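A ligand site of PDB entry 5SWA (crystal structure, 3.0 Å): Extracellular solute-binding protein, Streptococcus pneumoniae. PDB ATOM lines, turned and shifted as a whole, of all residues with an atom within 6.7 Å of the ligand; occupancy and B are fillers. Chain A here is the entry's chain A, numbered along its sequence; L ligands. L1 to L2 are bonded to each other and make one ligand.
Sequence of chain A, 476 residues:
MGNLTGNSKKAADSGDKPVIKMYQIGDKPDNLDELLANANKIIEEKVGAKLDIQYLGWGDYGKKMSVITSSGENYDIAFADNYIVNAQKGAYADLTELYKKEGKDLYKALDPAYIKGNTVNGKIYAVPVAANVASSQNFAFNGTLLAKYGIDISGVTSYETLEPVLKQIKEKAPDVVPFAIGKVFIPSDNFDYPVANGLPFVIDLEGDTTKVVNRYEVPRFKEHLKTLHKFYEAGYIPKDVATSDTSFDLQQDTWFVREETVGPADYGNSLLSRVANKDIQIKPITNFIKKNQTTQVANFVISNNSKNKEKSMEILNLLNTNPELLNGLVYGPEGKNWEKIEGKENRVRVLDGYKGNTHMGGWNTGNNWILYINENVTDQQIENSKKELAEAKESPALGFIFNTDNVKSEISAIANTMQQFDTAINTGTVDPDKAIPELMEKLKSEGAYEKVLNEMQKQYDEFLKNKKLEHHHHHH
O1 of LG2 L2 is in hydrogen-bond range of OG1 of Thr 261 (2.7 Å). OD1 of Asp 266 lies within hydrogen-bond range of O1 of LIG L1 (2.9 Å). The side-chain amide nitrogen of Asn 132 is in hydrogen-bond range of an oxygen (O5) of LIG L1 (3.2 Å).
OG1 of Thr 261 is in hydrogen-bond range of OE1 of Gln 137. The side-chain amide nitrogen of Asn 132 lies within hydrogen-bond range of the side-chain carboxylate of Asp 266 (3.2 Å). The backbone carbonyl oxygen (O) of Asp 266 sits at hydrogen-bond distance from the backbone NH (N) of Leu 271 (3.3 Å). The side-chain carboxylate (OD2) of Asp 266 lies within hydrogen-bond range of the backbone NH (N) of Gly 263, at 2.8 Å. The side-chain amide nitrogen (ND2) of Asn 132 lies close to the backbone NH (N) of Gly 263 (3.4 Å). OD1 of Asn 132 is in hydrogen-bond range of N of Ala 265, 3.1 Å away.
Residues that only touch the ligand: Trp 363 (3.5 Å), Val 297 (3.7 Å), Leu 271 (3.9 Å) and Trp 58 (3.97 Å). Hydrophobic or aromatic side chains that line the ligand: Trp 58, Leu 271, Val 297 and Trp 363. Of the 26 residues printed, 7 come within 4 Å of the ligand. Along chain A the residues within 4 Å of the ligand span positions 58 to 363. The nearest printed residue that does not touch the ligand is Glu 260 (4.1 Å).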
ATOM      1  N   ILE A  25     -26.149  17.439  -0.626  1.00  0.00           N
ATOM      2  CA  ILE A  25     -25.177  18.153   0.213  1.00  0.00           C
ATOM      3  C   ILE A  25     -25.866  19.237   1.044  1.00  0.00           C
ATOM      4  O   ILE A  25     -26.849  19.845   0.610  1.00  0.00           O
ATOM      5  CB  ILE A  25     -24.020  18.766  -0.634  1.00  0.00           C
ATOM      6  CG1 ILE A  25     -22.862  19.224   0.276  1.00  0.00           C
ATOM      7  CG2 ILE A  25     -24.526  19.888  -1.535  1.00  0.00           C
ATOM      8  CD1 ILE A  25     -21.666  19.784  -0.455  1.00  0.00           C
ATOM      9  N   TRP A  58     -22.429  19.420   5.421  1.00  0.00           N
ATOM     10  CA  TRP A  58     -21.490  20.228   4.652  1.00  0.00           C
ATOM     11  C   TRP A  58     -20.043  19.746   4.783  1.00  0.00           C
ATOM     12  O   TRP A  58     -19.520  19.084   3.892  1.00  0.00           O
ATOM     13  CB  TRP A  58     -21.582  21.703   5.046  1.00  0.00           C
ATOM     14  CG  TRP A  58     -22.710  22.437   4.397  1.00  0.00           C
ATOM     15  CD1 TRP A  58     -23.838  22.896   5.004  1.00  0.00           C
ATOM     16  CD2 TRP A  58     -22.806  22.796   3.016  1.00  0.00           C
ATOM     17  NE1 TRP A  58     -24.640  23.516   4.078  1.00  0.00           N
ATOM     18  CE2 TRP A  58     -24.035  23.470   2.847  1.00  0.00           C
ATOM     19  CE3 TRP A  58     -21.976  22.609   1.902  1.00  0.00           C
ATOM     20  CZ2 TRP A  58     -24.459  23.971   1.615  1.00  0.00           C
ATOM     21  CZ3 TRP A  58     -22.400  23.110   0.670  1.00  0.00           C
ATOM     22  CH2 TRP A  58     -23.632  23.777   0.541  1.00  0.00           C
ATOM     23  N   PHE A  79     -25.937  14.201  -5.291  1.00  0.00           N
ATOM     24  CA  PHE A  79     -25.184  15.405  -5.606  1.00  0.00           C
ATOM     25  C   PHE A  79     -23.737  14.986  -5.841  1.00  0.00           C
ATOM     26  O   PHE A  79     -23.113  14.365  -4.981  1.00  0.00           O
ATOM     27  CB  PHE A  79     -25.290  16.421  -4.471  1.00  0.00           C
ATOM     28  CG  PHE A  79     -24.592  17.730  -4.762  1.00  0.00           C
ATOM     29  CD1 PHE A  79     -23.295  17.951  -4.321  1.00  0.00           C
ATOM     30  CD2 PHE A  79     -25.242  18.732  -5.473  1.00  0.00           C
ATOM     31  CE1 PHE A  79     -22.651  19.151  -4.586  1.00  0.00           C
ATOM     32  CE2 PHE A  79     -24.598  19.932  -5.737  1.00  0.00           C
ATOM     33  CZ  PHE A  79     -23.307  20.138  -5.290  1.00  0.00           C
ATOM     34  N   ALA A 131     -28.106  27.059 -13.998  1.00  0.00           N
ATOM     35  CA  ALA A 131     -27.958  28.282 -13.210  1.00  0.00           C
ATOM     36  C   ALA A 131     -26.858  29.155 -13.791  1.00  0.00           C
ATOM     37  O   ALA A 131     -26.836  29.412 -14.997  1.00  0.00           O
ATOM     38  CB  ALA A 131     -27.675  27.948 -11.747  1.00  0.00           C
ATOM     39  N   ASN A 132     -25.928  29.599 -12.944  1.00  0.00           N
ATOM     40  CA  ASN A 132     -24.815  30.436 -13.376  1.00  0.00           C
ATOM     41  C   ASN A 132     -23.756  29.623 -14.105  1.00  0.00           C
ATOM     42  O   ASN A 132     -22.745  29.232 -13.516  1.00  0.00           O
ATOM     43  CB  ASN A 132     -24.183  31.144 -12.171  1.00  0.00           C
ATOM     44  CG  ASN A 132     -25.222  31.688 -11.214  1.00  0.00           C
ATOM     45  OD1 ASN A 132     -26.301  32.087 -11.624  1.00  0.00           O
ATOM     46  ND2 ASN A 132     -24.890  31.696  -9.928  1.00  0.00           N
ATOM     47  N   VAL A 133     -24.003  29.364 -15.389  1.00  0.00           N
ATOM     48  CA  VAL A 133     -23.021  28.687 -16.242  1.00  0.00           C
ATOM     49  C   VAL A 133     -21.773  29.584 -16.386  1.00  0.00           C
ATOM     50  O   VAL A 133     -20.676  29.101 -16.684  1.00  0.00           O
ATOM     51  CB  VAL A 133     -23.632  28.305 -17.611  1.00  0.00           C
ATOM     52  CG1 VAL A 133     -23.990  29.535 -18.428  1.00  0.00           C
ATOM     53  CG2 VAL A 133     -22.702  27.377 -18.382  1.00  0.00           C
ATOM     54  N   ALA A 134     -21.975  30.882 -16.167  1.00  0.00           N
ATOM     55  CA  ALA A 134     -20.882  31.831 -16.019  1.00  0.00           C
ATOM     56  C   ALA A 134     -21.091  32.604 -14.723  1.00  0.00           C
ATOM     57  O   ALA A 134     -22.224  32.965 -14.400  1.00  0.00           O
ATOM     58  CB  ALA A 134     -20.843  32.779 -17.200  1.00  0.00           C
ATOM     59  N   SER A 135     -20.016  32.855 -13.991  1.00  0.00           N
ATOM     60  CA  SER A 135     -20.089  33.550 -12.696  1.00  0.00           C
ATOM     61  C   SER A 135     -18.736  34.102 -12.252  1.00  0.00           C
ATOM     62  O   SER A 135     -17.695  33.723 -12.770  1.00  0.00           O
ATOM     63  CB  SER A 135     -20.652  32.615 -11.621  1.00  0.00           C
ATOM     64  OG  SER A 135     -19.838  31.465 -11.453  1.00  0.00           O
ATOM     65  N   GLN A 137     -16.367  35.591  -8.618  1.00  0.00           N
ATOM     66  CA  GLN A 137     -16.229  35.592  -7.167  1.00  0.00           C
ATOM     67  C   GLN A 137     -16.393  37.017  -6.676  1.00  0.00           C
ATOM     68  O   GLN A 137     -15.839  37.958  -7.261  1.00  0.00           O
ATOM     69  CB  GLN A 137     -14.880  35.001  -6.758  1.00  0.00           C
ATOM     70  CG  GLN A 137     -14.716  33.540  -7.153  1.00  0.00           C
ATOM     71  CD  GLN A 137     -15.775  32.657  -6.520  1.00  0.00           C
ATOM     72  OE1 GLN A 137     -16.748  32.276  -7.166  1.00  0.00           O
ATOM     73  NE2 GLN A 137     -15.602  32.363  -5.243  1.00  0.00           N
ATOM     74  N   GLU A 259     -16.901  35.898   0.932  1.00  0.00           N
ATOM     75  CA  GLU A 259     -16.785  35.682  -0.495  1.00  0.00           C
ATOM     76  C   GLU A 259     -17.862  34.734  -0.998  1.00  0.00           C
ATOM     77  O   GLU A 259     -18.119  33.702  -0.393  1.00  0.00           O
ATOM     78  CB  GLU A 259     -15.405  35.169  -0.865  1.00  0.00           C
ATOM     79  CG  GLU A 259     -15.207  34.990  -2.350  1.00  0.00           C
ATOM     80  CD  GLU A 259     -13.815  34.511  -2.682  1.00  0.00           C
ATOM     81  OE1 GLU A 259     -12.844  35.154  -2.224  1.00  0.00           O
ATOM     82  OE2 GLU A 259     -13.691  33.492  -3.398  1.00  0.00           O
ATOM     83  N   GLU A 260     -18.484  35.087  -2.111  1.00  0.00           N
ATOM     84  CA  GLU A 260     -19.575  34.310  -2.676  1.00  0.00           C
ATOM     85  C   GLU A 260     -19.420  34.158  -4.180  1.00  0.00           C
ATOM     86  O   GLU A 260     -18.803  34.996  -4.850  1.00  0.00           O
ATOM     87  CB  GLU A 260     -20.914  35.000  -2.382  1.00  0.00           C
ATOM     88  CG  GLU A 260     -21.428  34.807  -0.962  1.00  0.00           C
ATOM     89  CD  GLU A 260     -22.150  33.488  -0.767  1.00  0.00           C
ATOM     90  OE1 GLU A 260     -22.231  32.681  -1.718  1.00  0.00           O
ATOM     91  OE2 GLU A 260     -22.654  33.261   0.361  1.00  0.00           O
ATOM     92  N   THR A 261     -19.977  33.068  -4.714  1.00  0.00           N
ATOM     93  CA  THR A 261     -20.120  32.903  -6.144  1.00  0.00           C
ATOM     94  C   THR A 261     -21.456  33.534  -6.544  1.00  0.00           C
ATOM     95  O   THR A 261     -22.520  33.120  -6.061  1.00  0.00           O
ATOM     96  CB  THR A 261     -20.089  31.425  -6.565  1.00  0.00           C
ATOM     97  OG1 THR A 261     -18.922  30.793  -6.027  1.00  0.00           O
ATOM     98  CG2 THR A 261     -20.071  31.286  -8.089  1.00  0.00           C
ATOM     99  N   VAL A 262     -21.389  34.542  -7.405  1.00  0.00           N
ATOM    100  CA  VAL A 262     -22.579  35.264  -7.858  1.00  0.00           C
ATOM    101  C   VAL A 262     -22.722  35.157  -9.380  1.00  0.00           C
ATOM    102  O   VAL A 262     -21.730  35.243 -10.103  1.00  0.00           O
ATOM    103  CB  VAL A 262     -22.537  36.757  -7.448  1.00  0.00           C
ATOM    104  CG1 VAL A 262     -23.885  37.427  -7.690  1.00  0.00           C
ATOM    105  CG2 VAL A 262     -22.122  36.907  -5.997  1.00  0.00           C
ATOM    106  N   GLY A 263     -23.954  34.971  -9.839  1.00  0.00           N
ATOM    107  CA  GLY A 263     -24.208  34.831 -11.274  1.00  0.00           C
ATOM    108  C   GLY A 263     -25.516  35.430 -11.749  1.00  0.00           C
ATOM    109  O   GLY A 263     -26.228  36.060 -10.973  1.00  0.00           O
ATOM    110  N   ALA A 265     -28.371  34.082 -12.717  1.00  0.00           N
ATOM    111  CA  ALA A 265     -29.601  33.499 -12.177  1.00  0.00           C
ATOM    112  C   ALA A 265     -29.892  34.002 -10.774  1.00  0.00           C
ATOM    113  O   ALA A 265     -30.901  33.645 -10.183  1.00  0.00           O
ATOM    114  CB  ALA A 265     -29.520  31.976 -12.183  1.00  0.00           C
ATOM    115  N   ASP A 266     -28.990  34.837 -10.246  1.00  0.00           N
ATOM    116  CA  ASP A 266     -29.163  35.458  -8.943  1.00  0.00           C
ATOM    117  C   ASP A 266     -29.670  36.890  -9.073  1.00  0.00           C
ATOM    118  O   ASP A 266     -30.206  37.457  -8.108  1.00  0.00           O
ATOM    119  CB  ASP A 266     -27.836  35.447  -8.175  1.00  0.00           C
ATOM    120  CG  ASP A 266     -27.150  34.090  -8.189  1.00  0.00           C
ATOM    121  OD1 ASP A 266     -27.854  33.059  -8.297  1.00  0.00           O
ATOM    122  OD2 ASP A 266     -25.912  34.060  -8.086  1.00  0.00           O
ATOM    123  N   LEU A 271     -30.858  37.956  -4.881  1.00  0.00           N
ATOM    124  CA  LEU A 271     -30.989  36.717  -4.119  1.00  0.00           C
ATOM    125  C   LEU A 271     -30.228  36.775  -2.797  1.00  0.00           C
ATOM    126  O   LEU A 271     -30.724  36.286  -1.777  1.00  0.00           O
ATOM    127  CB  LEU A 271     -30.522  35.512  -4.951  1.00  0.00           C
ATOM    128  CG  LEU A 271     -30.442  34.166  -4.211  1.00  0.00           C
ATOM    129  CD1 LEU A 271     -31.812  33.739  -3.675  1.00  0.00           C
ATOM    130  CD2 LEU A 271     -29.852  33.074  -5.093  1.00  0.00           C
ATOM    131  N   LEU A 272     -29.041  37.356  -2.831  1.00  0.00           N
ATOM    132  CA  LEU A 272     -28.241  37.540  -1.624  1.00  0.00           C
ATOM    133  C   LEU A 272     -28.962  38.398  -0.582  1.00  0.00           C
ATOM    134  O   LEU A 272     -28.979  38.046   0.597  1.00  0.00           O
ATOM    135  CB  LEU A 272     -26.872  38.130  -1.957  1.00  0.00           C
ATOM    136  CG  LEU A 272     -25.792  37.087  -2.257  1.00  0.00           C
ATOM    137  CD1 LEU A 272     -24.557  37.725  -2.847  1.00  0.00           C
ATOM    138  CD2 LEU A 272     -25.443  36.330  -0.987  1.00  0.00           C
ATOM    139  N   VAL A 275     -32.159  36.228   0.964  1.00  0.00           N
ATOM    140  CA  VAL A 275     -31.900  35.195   1.951  1.00  0.00           C
ATOM    141  C   VAL A 275     -31.337  35.801   3.244  1.00  0.00           C
ATOM    142  O   VAL A 275     -31.457  35.210   4.309  1.00  0.00           O
ATOM    143  CB  VAL A 275     -30.957  34.107   1.407  1.00  0.00           C
ATOM    144  CG1 VAL A 275     -31.595  33.405   0.222  1.00  0.00           C
ATOM    145  CG2 VAL A 275     -29.614  34.704   1.012  1.00  0.00           C
ATOM    146  N   THR A 294     -17.647  26.293 -13.441  1.00  0.00           N
ATOM    147  CA  THR A 294     -18.990  26.869 -13.393  1.00  0.00           C
ATOM    148  C   THR A 294     -20.051  25.883 -13.881  1.00  0.00           C
ATOM    149  O   THR A 294     -21.205  25.936 -13.442  1.00  0.00           O
ATOM    150  CB  THR A 294     -19.074  28.178 -14.202  1.00  0.00           C
ATOM    151  OG1 THR A 294     -18.328  28.063 -15.412  1.00  0.00           O
ATOM    152  CG2 THR A 294     -18.520  29.341 -13.399  1.00  0.00           C
ATOM    153  N   VAL A 297     -20.423  22.897 -11.123  1.00  0.00           N
ATOM    154  CA  VAL A 297     -20.612  23.412  -9.760  1.00  0.00           C
ATOM    155  C   VAL A 297     -21.766  22.738  -9.026  1.00  0.00           C
ATOM    156  O   VAL A 297     -21.793  22.722  -7.796  1.00  0.00           O
ATOM    157  CB  VAL A 297     -20.769  24.951  -9.747  1.00  0.00           C
ATOM    158  CG1 VAL A 297     -22.199  25.361 -10.104  1.00  0.00           C
ATOM    159  CG2 VAL A 297     -20.387  25.514  -8.386  1.00  0.00           C
ATOM    160  N   ALA A 298     -22.720  22.189  -9.771  1.00  0.00           N
ATOM    161  CA  ALA A 298     -23.883  21.540  -9.176  1.00  0.00           C
ATOM    162  C   ALA A 298     -24.476  20.472 -10.077  1.00  0.00           C
ATOM    163  O   ALA A 298     -25.489  20.681 -10.740  1.00  0.00           O
ATOM    164  CB  ALA A 298     -24.942  22.586  -8.823  1.00  0.00           C
ATOM    165  N   GLY A 361     -32.139  25.513  -1.575  1.00  0.00           N
ATOM    166  CA  GLY A 361     -31.387  26.423  -2.445  1.00  0.00           C
ATOM    167  C   GLY A 361     -31.611  26.088  -3.913  1.00  0.00           C
ATOM    168  O   GLY A 361     -31.604  24.907  -4.292  1.00  0.00           O
ATOM    169  N   GLY A 362     -31.817  27.113  -4.734  1.00  0.00           N
ATOM    170  CA  GLY A 362     -32.109  26.931  -6.160  1.00  0.00           C
ATOM    171  C   GLY A 362     -30.953  26.429  -7.007  1.00  0.00           C
ATOM    172  O   GLY A 362     -31.159  25.711  -7.993  1.00  0.00           O
ATOM    173  N   TRP A 363     -29.734  26.810  -6.616  1.00  0.00           N
ATOM    174  CA  TRP A 363     -28.529  26.477  -7.366  1.00  0.00           C
ATOM    175  C   TRP A 363     -28.251  24.979  -7.412  1.00  0.00           C
ATOM    176  O   TRP A 363     -27.557  24.504  -8.315  1.00  0.00           O
ATOM    177  CB  TRP A 363     -27.323  27.219  -6.788  1.00  0.00           C
ATOM    178  CG  TRP A 363     -26.927  26.752  -5.420  1.00  0.00           C
ATOM    179  CD1 TRP A 363     -27.528  27.065  -4.232  1.00  0.00           C
ATOM    180  CD2 TRP A 363     -25.856  25.854  -5.092  1.00  0.00           C
ATOM    181  NE1 TRP A 363     -26.889  26.438  -3.188  1.00  0.00           N
ATOM    182  CE2 TRP A 363     -25.857  25.691  -3.683  1.00  0.00           C
ATOM    183  CE3 TRP A 363     -24.881  25.183  -5.853  1.00  0.00           C
ATOM    184  CZ2 TRP A 363     -24.929  24.879  -3.025  1.00  0.00           C
ATOM    185  CZ3 TRP A 363     -23.962  24.389  -5.193  1.00  0.00           C
ATOM    186  CH2 TRP A 363     -23.998  24.231  -3.786  1.00  0.00           C
ATOM    187  N   ASN A 368     -32.834  27.091 -12.644  1.00  0.00           N
ATOM    188  CA  ASN A 368     -32.961  28.415 -12.025  1.00  0.00           C
ATOM    189  C   ASN A 368     -33.824  29.384 -12.842  1.00  0.00           C
ATOM    190  O   ASN A 368     -34.139  30.481 -12.394  1.00  0.00           O
ATOM    191  CB  ASN A 368     -31.582  29.031 -11.781  1.00  0.00           C
ATOM    192  CG  ASN A 368     -30.919  28.508 -10.512  1.00  0.00           C
ATOM    193  OD1 ASN A 368     -30.353  29.277  -9.740  1.00  0.00           O
ATOM    194  ND2 ASN A 368     -30.950  27.193 -10.306  1.00  0.00           N
HETATM  195  C1  LIG L   1     -25.356  30.712  -6.455  1.00  0.00           C
HETATM  196  C2  LIG L   1     -25.223  30.186  -5.030  1.00  0.00           C
HETATM  197  C3  LIG L   1     -23.769  29.838  -4.791  1.00  0.00           C
HETATM  198  C4  LIG L   1     -23.224  28.905  -5.843  1.00  0.00           C
HETATM  199  C5  LIG L   1     -23.500  29.478  -7.221  1.00  0.00           C
HETATM  200  C6  LIG L   1     -23.046  28.477  -8.273  1.00  0.00           C
HETATM  201  C7  LIG L   1     -26.536  31.286  -3.230  1.00  0.00           C
HETATM  202  C8  LIG L   1     -26.452  32.485  -2.330  1.00  0.00           C
HETATM  203  N1  LIG L   1     -25.487  31.189  -4.043  1.00  0.00           N
HETATM  204  O1  LIG L   1     -26.712  30.975  -6.710  1.00  0.00           O
HETATM  205  O2  LIG L   1     -23.605  29.216  -3.534  1.00  0.00           O
HETATM  206  O3  LIG L   1     -21.828  28.815  -5.644  1.00  0.00           O
HETATM  207  O4  LIG L   1     -24.880  29.723  -7.349  1.00  0.00           O
HETATM  208  O5  LIG L   1     -23.291  28.995  -9.556  1.00  0.00           O
HETATM  209  O6  LIG L   1     -27.533  30.545  -3.147  1.00  0.00           O
HETATM  210  C1  LG2 L   2     -21.503  27.636  -4.903  1.00  0.00           C
HETATM  211  C2  LG2 L   2     -20.047  27.281  -5.166  1.00  0.00           C
HETATM  212  C3  LG2 L   2     -19.624  26.043  -4.375  1.00  0.00           C
HETATM  213  C4  LG2 L   2     -20.028  26.145  -2.913  1.00  0.00           C
HETATM  214  C5  LG2 L   2     -21.481  26.585  -2.766  1.00  0.00           C
HETATM  215  C6  LG2 L   2     -21.838  26.800  -1.299  1.00  0.00           C
HETATM  216  O1  LG2 L   2     -19.207  28.378  -4.799  1.00  0.00           O
HETATM  217  O2  LG2 L   2     -18.201  25.882  -4.463  1.00  0.00           O
HETATM  218  O3  LG2 L   2     -19.851  24.875  -2.292  1.00  0.00           O
HETATM  219  O4  LG2 L   2     -21.690  27.797  -3.492  1.00  0.00           O
HETATM  220  O5  LG2 L   2     -21.544  28.153  -0.924  1.00  0.00           O
